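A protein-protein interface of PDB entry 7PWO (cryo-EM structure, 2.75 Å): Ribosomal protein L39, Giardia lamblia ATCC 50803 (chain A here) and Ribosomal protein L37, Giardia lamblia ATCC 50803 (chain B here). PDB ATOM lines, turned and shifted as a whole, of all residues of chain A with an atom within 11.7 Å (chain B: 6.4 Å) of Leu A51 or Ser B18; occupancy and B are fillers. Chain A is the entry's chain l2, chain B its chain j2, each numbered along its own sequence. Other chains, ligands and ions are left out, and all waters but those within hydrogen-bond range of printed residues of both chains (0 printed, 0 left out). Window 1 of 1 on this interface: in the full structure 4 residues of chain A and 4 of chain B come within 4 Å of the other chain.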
ATOM      1  N   THR A   2      -9.756  36.917  -5.754  1.00  0.00           N
ATOM      2  CA  THR A   2      -9.895  37.321  -4.358  1.00  0.00           C
ATOM      3  C   THR A   2      -8.535  37.753  -3.817  1.00  0.00           C
ATOM      4  O   THR A   2      -7.507  37.317  -4.310  1.00  0.00           O
ATOM      5  CB  THR A   2     -10.510  36.164  -3.502  1.00  0.00           C
ATOM      6  OG1 THR A   2     -10.700  36.576  -2.143  1.00  0.00           O
ATOM      7  CG2 THR A   2      -9.640  34.922  -3.527  1.00  0.00           C
ATOM      8  N   ASN A   4      -7.708  37.007  -0.750  1.00  0.00           N
ATOM      9  CA  ASN A   4      -7.469  36.036   0.319  1.00  0.00           C
ATOM     10  C   ASN A   4      -7.546  34.638  -0.276  1.00  0.00           C
ATOM     11  O   ASN A   4      -8.581  33.981  -0.201  1.00  0.00           O
ATOM     12  CB  ASN A   4      -8.509  36.225   1.443  1.00  0.00           C
ATOM     13  CG  ASN A   4      -8.660  37.658   1.862  1.00  0.00           C
ATOM     14  OD1 ASN A   4      -7.842  38.193   2.600  1.00  0.00           O
ATOM     15  ND2 ASN A   4      -9.709  38.292   1.392  1.00  0.00           N
ATOM     16  N   LYS A   5      -6.442  34.164  -0.834  1.00  0.00           N
ATOM     17  CA  LYS A   5      -6.452  32.917  -1.581  1.00  0.00           C
ATOM     18  C   LYS A   5      -5.399  31.957  -1.045  1.00  0.00           C
ATOM     19  O   LYS A   5      -4.327  32.371  -0.604  1.00  0.00           O
ATOM     20  CB  LYS A   5      -6.230  33.173  -3.087  1.00  0.00           C
ATOM     21  CG  LYS A   5      -4.830  33.601  -3.478  1.00  0.00           C
ATOM     22  CD  LYS A   5      -4.621  33.497  -4.988  1.00  0.00           C
ATOM     23  CE  LYS A   5      -5.150  34.690  -5.773  1.00  0.00           C
ATOM     24  NZ  LYS A   5      -4.842  35.996  -5.161  1.00  0.00           N
ATOM     25  N   THR A   6      -5.727  30.667  -1.080  1.00  0.00           N
ATOM     26  CA  THR A   6      -4.802  29.623  -0.652  1.00  0.00           C
ATOM     27  C   THR A   6      -3.645  29.465  -1.635  1.00  0.00           C
ATOM     28  O   THR A   6      -3.756  29.770  -2.825  1.00  0.00           O
ATOM     29  CB  THR A   6      -5.524  28.275  -0.496  1.00  0.00           C
ATOM     30  OG1 THR A   6      -5.873  27.753  -1.782  1.00  0.00           O
ATOM     31  CG2 THR A   6      -6.778  28.401   0.348  1.00  0.00           C
ATOM     32  N   LEU A   7      -2.530  28.948  -1.116  1.00  0.00           N
ATOM     33  CA  LEU A   7      -1.323  28.778  -1.917  1.00  0.00           C
ATOM     34  C   LEU A   7      -1.522  27.801  -3.072  1.00  0.00           C
ATOM     35  O   LEU A   7      -0.927  27.981  -4.134  1.00  0.00           O
ATOM     36  CB  LEU A   7      -0.170  28.329  -1.014  1.00  0.00           C
ATOM     37  CG  LEU A   7       1.280  28.314  -1.515  1.00  0.00           C
ATOM     38  CD1 LEU A   7       1.731  29.680  -1.984  1.00  0.00           C
ATOM     39  CD2 LEU A   7       2.202  27.779  -0.433  1.00  0.00           C
ATOM     40  N   SER A   8      -2.360  26.779  -2.902  1.00  0.00           N
ATOM     41  CA  SER A   8      -2.577  25.823  -3.988  1.00  0.00           C
ATOM     42  C   SER A   8      -3.275  26.467  -5.183  1.00  0.00           C
ATOM     43  O   SER A   8      -2.867  26.264  -6.338  1.00  0.00           O
ATOM     44  CB  SER A   8      -3.380  24.636  -3.476  1.00  0.00           C
ATOM     45  OG  SER A   8      -2.567  23.798  -2.695  1.00  0.00           O
ATOM     46  N   ARG A   9      -4.318  27.257  -4.924  1.00  0.00           N
ATOM     47  CA  ARG A   9      -4.972  27.987  -6.003  1.00  0.00           C
ATOM     48  C   ARG A   9      -4.039  29.028  -6.600  1.00  0.00           C
ATOM     49  O   ARG A   9      -4.008  29.212  -7.826  1.00  0.00           O
ATOM     50  CB  ARG A   9      -6.267  28.622  -5.501  1.00  0.00           C
ATOM     51  CG  ARG A   9      -7.361  27.614  -5.176  1.00  0.00           C
ATOM     52  CD  ARG A   9      -8.680  28.279  -4.794  1.00  0.00           C
ATOM     53  NE  ARG A   9      -9.382  28.866  -5.930  1.00  0.00           N
ATOM     54  CZ  ARG A   9     -10.172  29.934  -5.862  1.00  0.00           C
ATOM     55  NH1 ARG A   9     -10.761  30.398  -6.956  1.00  0.00           N
ATOM     56  NH2 ARG A   9     -10.383  30.535  -4.706  1.00  0.00           N
ATOM     57  N   LYS A  10      -3.239  29.685  -5.752  1.00  0.00           N
ATOM     58  CA  LYS A  10      -2.240  30.621  -6.253  1.00  0.00           C
ATOM     59  C   LYS A  10      -1.291  29.951  -7.239  1.00  0.00           C
ATOM     60  O   LYS A  10      -1.003  30.510  -8.300  1.00  0.00           O
ATOM     61  CB  LYS A  10      -1.456  31.228  -5.092  1.00  0.00           C
ATOM     62  CG  LYS A  10      -0.678  32.493  -5.413  1.00  0.00           C
ATOM     63  CD  LYS A  10      -0.070  33.051  -4.144  1.00  0.00           C
ATOM     64  CE  LYS A  10       1.037  34.047  -4.404  1.00  0.00           C
ATOM     65  NZ  LYS A  10       1.310  34.846  -3.194  1.00  0.00           N
ATOM     66  N   LEU A  11      -0.809  28.749  -6.917  1.00  0.00           N
ATOM     67  CA  LEU A  11       0.181  28.097  -7.772  1.00  0.00           C
ATOM     68  C   LEU A  11      -0.420  27.635  -9.092  1.00  0.00           C
ATOM     69  O   LEU A  11       0.216  27.762 -10.148  1.00  0.00           O
ATOM     70  CB  LEU A  11       0.832  26.929  -7.038  1.00  0.00           C
ATOM     71  CG  LEU A  11       1.701  27.325  -5.843  1.00  0.00           C
ATOM     72  CD1 LEU A  11       1.976  26.156  -4.892  1.00  0.00           C
ATOM     73  CD2 LEU A  11       2.989  27.961  -6.305  1.00  0.00           C
ATOM     74  N   ARG A  12      -1.635  27.091  -9.071  1.00  0.00           N
ATOM     75  CA  ARG A  12      -2.210  26.680 -10.350  1.00  0.00           C
ATOM     76  C   ARG A  12      -2.516  27.890 -11.244  1.00  0.00           C
ATOM     77  O   ARG A  12      -2.250  27.864 -12.462  1.00  0.00           O
ATOM     78  CB  ARG A  12      -3.433  25.799 -10.108  1.00  0.00           C
ATOM     79  CG  ARG A  12      -3.058  24.433  -9.516  1.00  0.00           C
ATOM     80  CD  ARG A  12      -4.210  23.461  -9.576  1.00  0.00           C
ATOM     81  NE  ARG A  12      -4.449  22.976 -10.931  1.00  0.00           N
ATOM     82  CZ  ARG A  12      -5.127  21.876 -11.231  1.00  0.00           C
ATOM     83  NH1 ARG A  12      -5.655  21.134 -10.280  1.00  0.00           N
ATOM     84  NH2 ARG A  12      -5.291  21.529 -12.495  1.00  0.00           N
ATOM     85  N   LEU A  13      -3.018  28.982 -10.656  1.00  0.00           N
ATOM     86  CA  LEU A  13      -3.194  30.221 -11.410  1.00  0.00           C
ATOM     87  C   LEU A  13      -1.866  30.734 -11.958  1.00  0.00           C
ATOM     88  O   LEU A  13      -1.793  31.213 -13.102  1.00  0.00           O
ATOM     89  CB  LEU A  13      -3.854  31.274 -10.522  1.00  0.00           C
ATOM     90  CG  LEU A  13      -5.361  31.122 -10.310  1.00  0.00           C
ATOM     91  CD1 LEU A  13      -5.918  32.276  -9.495  1.00  0.00           C
ATOM     92  CD2 LEU A  13      -6.096  30.979 -11.626  1.00  0.00           C
ATOM     93  N   ALA A  14      -0.805  30.632 -11.157  1.00  0.00           N
ATOM     94  CA  ALA A  14       0.513  31.090 -11.577  1.00  0.00           C
ATOM     95  C   ALA A  14       1.018  30.313 -12.780  1.00  0.00           C
ATOM     96  O   ALA A  14       1.647  30.885 -13.673  1.00  0.00           O
ATOM     97  CB  ALA A  14       1.496  30.961 -10.415  1.00  0.00           C
ATOM     98  N   LYS A  15       0.772  29.003 -12.814  1.00  0.00           N
ATOM     99  CA  LYS A  15       1.174  28.225 -13.981  1.00  0.00           C
ATOM    100  C   LYS A  15       0.399  28.629 -15.233  1.00  0.00           C
ATOM    101  O   LYS A  15       0.985  28.719 -16.320  1.00  0.00           O
ATOM    102  CB  LYS A  15       1.014  26.732 -13.724  1.00  0.00           C
ATOM    103  CG  LYS A  15       1.644  25.887 -14.803  1.00  0.00           C
ATOM    104  CD  LYS A  15       0.989  24.538 -14.926  1.00  0.00           C
ATOM    105  CE  LYS A  15       1.670  23.709 -16.006  1.00  0.00           C
ATOM    106  NZ  LYS A  15       1.008  22.397 -16.205  1.00  0.00           N
ATOM    107  N   LYS A  16      -0.915  28.854 -15.122  1.00  0.00           N
ATOM    108  CA  LYS A  16      -1.649  29.313 -16.308  1.00  0.00           C
ATOM    109  C   LYS A  16      -1.061  30.618 -16.847  1.00  0.00           C
ATOM    110  O   LYS A  16      -0.803  30.753 -18.056  1.00  0.00           O
ATOM    111  CB  LYS A  16      -3.136  29.491 -15.998  1.00  0.00           C
ATOM    112  CG  LYS A  16      -3.870  28.228 -15.597  1.00  0.00           C
ATOM    113  CD  LYS A  16      -3.909  27.210 -16.715  1.00  0.00           C
ATOM    114  CE  LYS A  16      -4.819  27.629 -17.840  1.00  0.00           C
ATOM    115  NZ  LYS A  16      -4.885  26.563 -18.890  1.00  0.00           N
ATOM    116  N   THR A  17      -0.804  31.577 -15.951  1.00  0.00           N
ATOM    117  CA  THR A  17      -0.197  32.841 -16.364  1.00  0.00           C
ATOM    118  C   THR A  17       1.164  32.625 -17.011  1.00  0.00           C
ATOM    119  O   THR A  17       1.485  33.247 -18.030  1.00  0.00           O
ATOM    120  CB  THR A  17      -0.059  33.784 -15.169  1.00  0.00           C
ATOM    121  OG1 THR A  17      -1.355  34.190 -14.724  1.00  0.00           O
ATOM    122  CG2 THR A  17       0.717  35.024 -15.564  1.00  0.00           C
ATOM    123  N   THR A  19       2.430  29.997 -18.597  1.00  0.00           N
ATOM    124  CA  THR A  19       2.444  29.309 -19.883  1.00  0.00           C
ATOM    125  C   THR A  19       1.616  30.006 -20.959  1.00  0.00           C
ATOM    126  O   THR A  19       1.616  29.546 -22.103  1.00  0.00           O
ATOM    127  CB  THR A  19       1.962  27.859 -19.721  1.00  0.00           C
ATOM    128  OG1 THR A  19       0.600  27.839 -19.277  1.00  0.00           O
ATOM    129  CG2 THR A  19       2.825  27.111 -18.727  1.00  0.00           C
ATOM    130  N   HIS A  42      -5.119  32.019 -23.799  1.00  0.00           N
ATOM    131  CA  HIS A  42      -6.408  32.448 -23.284  1.00  0.00           C
ATOM    132  C   HIS A  42      -6.318  33.917 -22.893  1.00  0.00           C
ATOM    133  O   HIS A  42      -5.234  34.445 -22.648  1.00  0.00           O
ATOM    134  CB  HIS A  42      -6.846  31.558 -22.108  1.00  0.00           C
ATOM    135  CG  HIS A  42      -5.943  31.631 -20.920  1.00  0.00           C
ATOM    136  ND1 HIS A  42      -5.650  32.807 -20.269  1.00  0.00           N
ATOM    137  CD2 HIS A  42      -5.192  30.680 -20.322  1.00  0.00           C
ATOM    138  CE1 HIS A  42      -4.799  32.571 -19.290  1.00  0.00           C
ATOM    139  NE2 HIS A  42      -4.502  31.288 -19.302  1.00  0.00           N
ATOM    140  N   SER A  47     -12.365  34.143 -20.779  1.00  0.00           N
ATOM    141  CA  SER A  47     -12.000  32.843 -20.240  1.00  0.00           C
ATOM    142  C   SER A  47     -12.832  32.497 -19.014  1.00  0.00           C
ATOM    143  O   SER A  47     -13.397  33.357 -18.339  1.00  0.00           O
ATOM    144  CB  SER A  47     -10.516  32.781 -19.878  1.00  0.00           C
ATOM    145  OG  SER A  47     -10.194  33.594 -18.769  1.00  0.00           O
ATOM    146  N   HIS A  48     -12.888  31.205 -18.739  1.00  0.00           N
ATOM    147  CA  HIS A  48     -13.531  30.636 -17.574  1.00  0.00           C
ATOM    148  C   HIS A  48     -12.619  29.607 -16.941  1.00  0.00           C
ATOM    149  O   HIS A  48     -13.010  28.463 -16.716  1.00  0.00           O
ATOM    150  CB  HIS A  48     -14.870  29.995 -17.925  1.00  0.00           C
ATOM    151  CG  HIS A  48     -15.854  30.939 -18.530  1.00  0.00           C
ATOM    152  ND1 HIS A  48     -16.624  31.792 -17.773  1.00  0.00           N
ATOM    153  CD2 HIS A  48     -16.190  31.168 -19.818  1.00  0.00           C
ATOM    154  CE1 HIS A  48     -17.400  32.502 -18.569  1.00  0.00           C
ATOM    155  NE2 HIS A  48     -17.152  32.148 -19.817  1.00  0.00           N
ATOM    156  N   LEU A  49     -11.355  29.973 -16.742  1.00  0.00           N
ATOM    157  CA  LEU A  49     -10.495  29.224 -15.837  1.00  0.00           C
ATOM    158  C   LEU A  49     -11.251  28.889 -14.568  1.00  0.00           C
ATOM    159  O   LEU A  49     -11.801  29.775 -13.909  1.00  0.00           O
ATOM    160  CB  LEU A  49      -9.237  30.030 -15.505  1.00  0.00           C
ATOM    161  CG  LEU A  49      -8.066  30.138 -16.467  1.00  0.00           C
ATOM    162  CD1 LEU A  49      -8.353  30.966 -17.667  1.00  0.00           C
ATOM    163  CD2 LEU A  49      -6.954  30.785 -15.691  1.00  0.00           C
ATOM    164  N   LYS A  50     -11.298  27.608 -14.241  1.00  0.00           N
ATOM    165  CA  LYS A  50     -12.044  27.153 -13.078  1.00  0.00           C
ATOM    166  C   LYS A  50     -11.063  26.607 -12.061  1.00  0.00           C
ATOM    167  O   LYS A  50     -11.240  25.506 -11.534  1.00  0.00           O
ATOM    168  CB  LYS A  50     -13.092  26.105 -13.460  1.00  0.00           C
ATOM    169  CG  LYS A  50     -14.232  26.633 -14.303  1.00  0.00           C
ATOM    170  CD  LYS A  50     -15.242  25.537 -14.615  1.00  0.00           C
ATOM    171  CE  LYS A  50     -16.371  26.050 -15.473  1.00  0.00           C
ATOM    172  NZ  LYS A  50     -17.361  25.003 -15.800  1.00  0.00           N
ATOM    173  N   LEU A  51      -9.993  27.356 -11.826  1.00  0.00           N
ATOM    174  CA  LEU A  51      -8.949  26.943 -10.907  1.00  0.00           C
ATOM    175  C   LEU A  51      -8.849  27.895  -9.712  1.00  0.00           C
ATOM    176  O   LEU A  51      -9.658  28.812  -9.550  1.00  0.00           O
ATOM    177  CB  LEU A  51      -7.603  26.863 -11.627  1.00  0.00           C
ATOM    178  CG  LEU A  51      -7.338  25.570 -12.404  1.00  0.00           C
ATOM    179  CD1 LEU A  51      -7.300  24.421 -11.438  1.00  0.00           C
ATOM    180  CD2 LEU A  51      -8.312  25.298 -13.546  1.00  0.00           C
ATOM    181  OXT LEU A  51      -7.950  27.772  -8.873  1.00  0.00           O
ATOM    182  N   ARG B  14     -18.559  29.185  -5.076  1.00  0.00           N
ATOM    183  CA  ARG B  14     -17.922  28.038  -5.711  1.00  0.00           C
ATOM    184  C   ARG B  14     -18.572  26.769  -5.172  1.00  0.00           C
ATOM    185  O   ARG B  14     -18.543  26.520  -3.967  1.00  0.00           O
ATOM    186  CB  ARG B  14     -16.418  28.041  -5.452  1.00  0.00           C
ATOM    187  CG  ARG B  14     -15.796  29.395  -5.718  1.00  0.00           C
ATOM    188  CD  ARG B  14     -14.306  29.363  -5.968  1.00  0.00           C
ATOM    189  NE  ARG B  14     -13.563  29.045  -4.756  1.00  0.00           N
ATOM    190  CZ  ARG B  14     -12.902  27.911  -4.554  1.00  0.00           C
ATOM    191  NH1 ARG B  14     -12.852  26.987  -5.507  1.00  0.00           N
ATOM    192  NH2 ARG B  14     -12.264  27.720  -3.412  1.00  0.00           N
ATOM    193  N   HIS B  16     -17.894  23.529  -6.601  1.00  0.00           N
ATOM    194  CA  HIS B  16     -16.873  22.503  -6.718  1.00  0.00           C
ATOM    195  C   HIS B  16     -15.496  23.148  -6.795  1.00  0.00           C
ATOM    196  O   HIS B  16     -15.355  24.284  -7.243  1.00  0.00           O
ATOM    197  CB  HIS B  16     -17.112  21.630  -7.955  1.00  0.00           C
ATOM    198  CG  HIS B  16     -18.404  20.871  -7.927  1.00  0.00           C
ATOM    199  ND1 HIS B  16     -19.603  21.427  -8.316  1.00  0.00           N
ATOM    200  CD2 HIS B  16     -18.682  19.598  -7.575  1.00  0.00           C
ATOM    201  CE1 HIS B  16     -20.564  20.532  -8.198  1.00  0.00           C
ATOM    202  NE2 HIS B  16     -20.031  19.411  -7.751  1.00  0.00           N
ATOM    203  N   GLY B  17     -14.481  22.406  -6.354  1.00  0.00           N
ATOM    204  CA  GLY B  17     -13.092  22.817  -6.456  1.00  0.00           C
ATOM    205  C   GLY B  17     -12.180  21.731  -7.001  1.00  0.00           C
ATOM    206  O   GLY B  17     -12.672  20.710  -7.479  1.00  0.00           O
ATOM    207  N   SER B  18     -10.865  21.929  -6.950  1.00  0.00           N
ATOM    208  CA  SER B  18      -9.933  20.945  -7.501  1.00  0.00           C
ATOM    209  C   SER B  18      -9.844  19.704  -6.626  1.00  0.00           C
ATOM    210  O   SER B  18      -9.730  19.800  -5.402  1.00  0.00           O
ATOM    211  CB  SER B  18      -8.540  21.549  -7.682  1.00  0.00           C
ATOM    212  OG  SER B  18      -8.457  22.313  -8.863  1.00  0.00           O
ATOM    213  N   CYS B  19      -9.896  18.539  -7.264  1.00  0.00           N
ATOM    214  CA  CYS B  19      -9.734  17.273  -6.573  1.00  0.00           C
ATOM    215  C   CYS B  19      -8.257  16.972  -6.363  1.00  0.00           C
ATOM    216  O   CYS B  19      -7.421  17.265  -7.221  1.00  0.00           O
ATOM    217  CB  CYS B  19     -10.393  16.147  -7.366  1.00  0.00           C
ATOM    218  SG  CYS B  19     -10.166  14.484  -6.698  1.00  0.00           S
ATOM    219  N   ARG B  20      -7.937  16.403  -5.201  1.00  0.00           N
ATOM    220  CA  ARG B  20      -6.563  16.021  -4.903  1.00  0.00           C
ATOM    221  C   ARG B  20      -6.125  14.752  -5.636  1.00  0.00           C
ATOM    222  O   ARG B  20      -4.927  14.565  -5.851  1.00  0.00           O
ATOM    223  CB  ARG B  20      -6.382  15.857  -3.395  1.00  0.00           C
ATOM    224  CG  ARG B  20      -6.847  14.540  -2.823  1.00  0.00           C
ATOM    225  CD  ARG B  20      -6.215  14.309  -1.477  1.00  0.00           C
ATOM    226  NE  ARG B  20      -6.812  15.168  -0.467  1.00  0.00           N
ATOM    227  CZ  ARG B  20      -6.448  15.194   0.805  1.00  0.00           C
ATOM    228  NH1 ARG B  20      -5.471  14.411   1.229  1.00  0.00           N
ATOM    229  NH2 ARG B  20      -7.056  16.007   1.651  1.00  0.00           N
ATOM    230  N   GLY B  23      -7.726  15.703 -10.043  1.00  0.00           N
ATOM    231  CA  GLY B  23      -7.323  17.016 -10.497  1.00  0.00           C
ATOM    232  C   GLY B  23      -8.385  17.844 -11.180  1.00  0.00           C
ATOM    233  O   GLY B  23      -8.074  18.937 -11.660  1.00  0.00           O
ATOM    234  N   LYS B  24      -9.621  17.373 -11.239  1.00  0.00           N
ATOM    235  CA  LYS B  24     -10.662  18.048 -11.996  1.00  0.00           C
ATOM    236  C   LYS B  24     -11.479  18.975 -11.107  1.00  0.00           C
ATOM    237  O   LYS B  24     -11.478  18.869  -9.882  1.00  0.00           O
ATOM    238  CB  LYS B  24     -11.574  17.032 -12.681  1.00  0.00           C
ATOM    239  CG  LYS B  24     -10.836  16.091 -13.610  1.00  0.00           C
ATOM    240  CD  LYS B  24     -11.658  15.707 -14.814  1.00  0.00           C
ATOM    241  CE  LYS B  24     -13.087  15.375 -14.427  1.00  0.00           C
ATOM    242  NZ  LYS B  24     -13.978  15.398 -15.608  1.00  0.00           N
ATOM    243  N   HIS B  25     -12.193  19.890 -11.756  1.00  0.00           N
ATOM    244  CA  HIS B  25     -13.063  20.848 -11.077  1.00  0.00           C
ATOM    245  C   HIS B  25     -14.363  20.166 -10.634  1.00  0.00           C
ATOM    246  O   HIS B  25     -15.465  20.531 -11.029  1.00  0.00           O
ATOM    247  CB  HIS B  25     -13.339  22.024 -12.004  1.00  0.00           C
ATOM    248  CG  HIS B  25     -14.233  23.064 -11.412  1.00  0.00           C
ATOM    249  ND1 HIS B  25     -15.432  23.425 -11.985  1.00  0.00           N
ATOM    250  CD2 HIS B  25     -14.093  23.839 -10.314  1.00  0.00           C
ATOM    251  CE1 HIS B  25     -16.005  24.358 -11.250  1.00  0.00           C
ATOM    252  NE2 HIS B  25     -15.213  24.628 -10.231  1.00  0.00           N
ATOM    253  N   SER B  26     -14.218  19.146  -9.791  1.00  0.00           N
ATOM    254  CA  SER B  26     -15.332  18.264  -9.467  1.00  0.00           C
ATOM    255  C   SER B  26     -15.465  17.929  -7.990  1.00  0.00           C
ATOM    256  O   SER B  26     -16.354  17.151  -7.636  1.00  0.00           O
ATOM    257  CB  SER B  26     -15.218  16.945 -10.243  1.00  0.00           C
ATOM    258  OG  SER B  26     -15.049  17.163 -11.619  1.00  0.00           O
ATOM    259  N   PHE B  27     -14.616  18.458  -7.125  1.00  0.00           N
ATOM    260  CA  PHE B  27     -14.655  18.098  -5.715  1.00  0.00           C
ATOM    261  C   PHE B  27     -15.651  19.008  -5.003  1.00  0.00           C
ATOM    262  O   PHE B  27     -15.468  20.225  -4.969  1.00  0.00           O
ATOM    263  CB  PHE B  27     -13.269  18.217  -5.095  1.00  0.00           C
ATOM    264  CG  PHE B  27     -13.196  17.727  -3.694  1.00  0.00           C
ATOM    265  CD1 PHE B  27     -13.251  16.376  -3.427  1.00  0.00           C
ATOM    266  CD2 PHE B  27     -13.085  18.607  -2.638  1.00  0.00           C
ATOM    267  CE1 PHE B  27     -13.185  15.913  -2.147  1.00  0.00           C
ATOM    268  CE2 PHE B  27     -13.017  18.146  -1.353  1.00  0.00           C
ATOM    269  CZ  PHE B  27     -13.066  16.795  -1.108  1.00  0.00           C
ATOM    270  N   LEU B  29     -17.267  21.074  -2.357  1.00  0.00           N
ATOM    271  CA  LEU B  29     -16.650  21.710  -1.202  1.00  0.00           C
ATOM    272  C   LEU B  29     -17.506  21.643   0.053  1.00  0.00           C
ATOM    273  O   LEU B  29     -16.990  21.897   1.142  1.00  0.00           O
ATOM    274  CB  LEU B  29     -16.309  23.171  -1.522  1.00  0.00           C
ATOM    275  CG  LEU B  29     -15.485  23.461  -2.778  1.00  0.00           C
ATOM    276  CD1 LEU B  29     -15.364  24.943  -3.022  1.00  0.00           C
ATOM    277  CD2 LEU B  29     -14.109  22.840  -2.707  1.00  0.00           C
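The side-chain hydroxyl (OG) of Ser B18 lies within hydrogen-bond range of the guanidinium group (NH1) of Arg A12, 3.4 Å away.
NH1 of Arg A9 lies within salt-bridge range of O of Leu A51 (3.2 Å).
A ring nitrogen (NE2) of His B25 sits at hydrogen-bond distance from the backbone carbonyl oxygen of His B16 (3.0 Å).
Arg B14 touches Arg A9 (NE to NH2, 3.5 Å).
NH1 of Arg A12 touches O of Gly B23, 3.5 Å away.
CD of Lys A50 touches ND1 of His B25 (3.4 Å).
Leu A51 touches Ser B18.
Leu A51 touches one residue of chain B.
Ser B18 touches just these residues of chain A: Arg A12 and Leu A51.
No residue of chain A comes within 4 Å of Gly B17.
No residue of chain A comes within 4 Å of Ser B26.
Phe B27 touches none of the printed residues of chain A.
Of the printed residues of chain B, Arg A9 touches Arg B14.
Of the printed residues of chain A, Arg B14 touches Arg A9 (3.5 Å).
Of the printed residues of chain B, Lys A50 touches His B25 (3.4 Å).
Lys A16 touches none of the printed residues of chain B.
Ala A14 touches none of the printed residues of chain B.
The nearest residue of chain A that does not touch Ser B18 is Lys A50 (5.0 Å).
The nearest printed residue of chain B that does not touch Lys A50 is Ser B18 (5.0 Å).
Printed residues of chain B that touch a printed residue of chain A: Arg B14, Ser B18, Gly B23 and His B25.
Hydrophobic or aromatic side chains of chain B within 4 Å of the printed part of chain A: His B25.
Of the 22 printed residues of chain A, 4 touch a printed residue of chain B.
Among the printed residues, 5 pairs touch across the chains.
Among the printed residues, no Asp or Glu carboxylate lies within 4 Å of a Lys or Arg side-chain nitrogen of the other chain.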
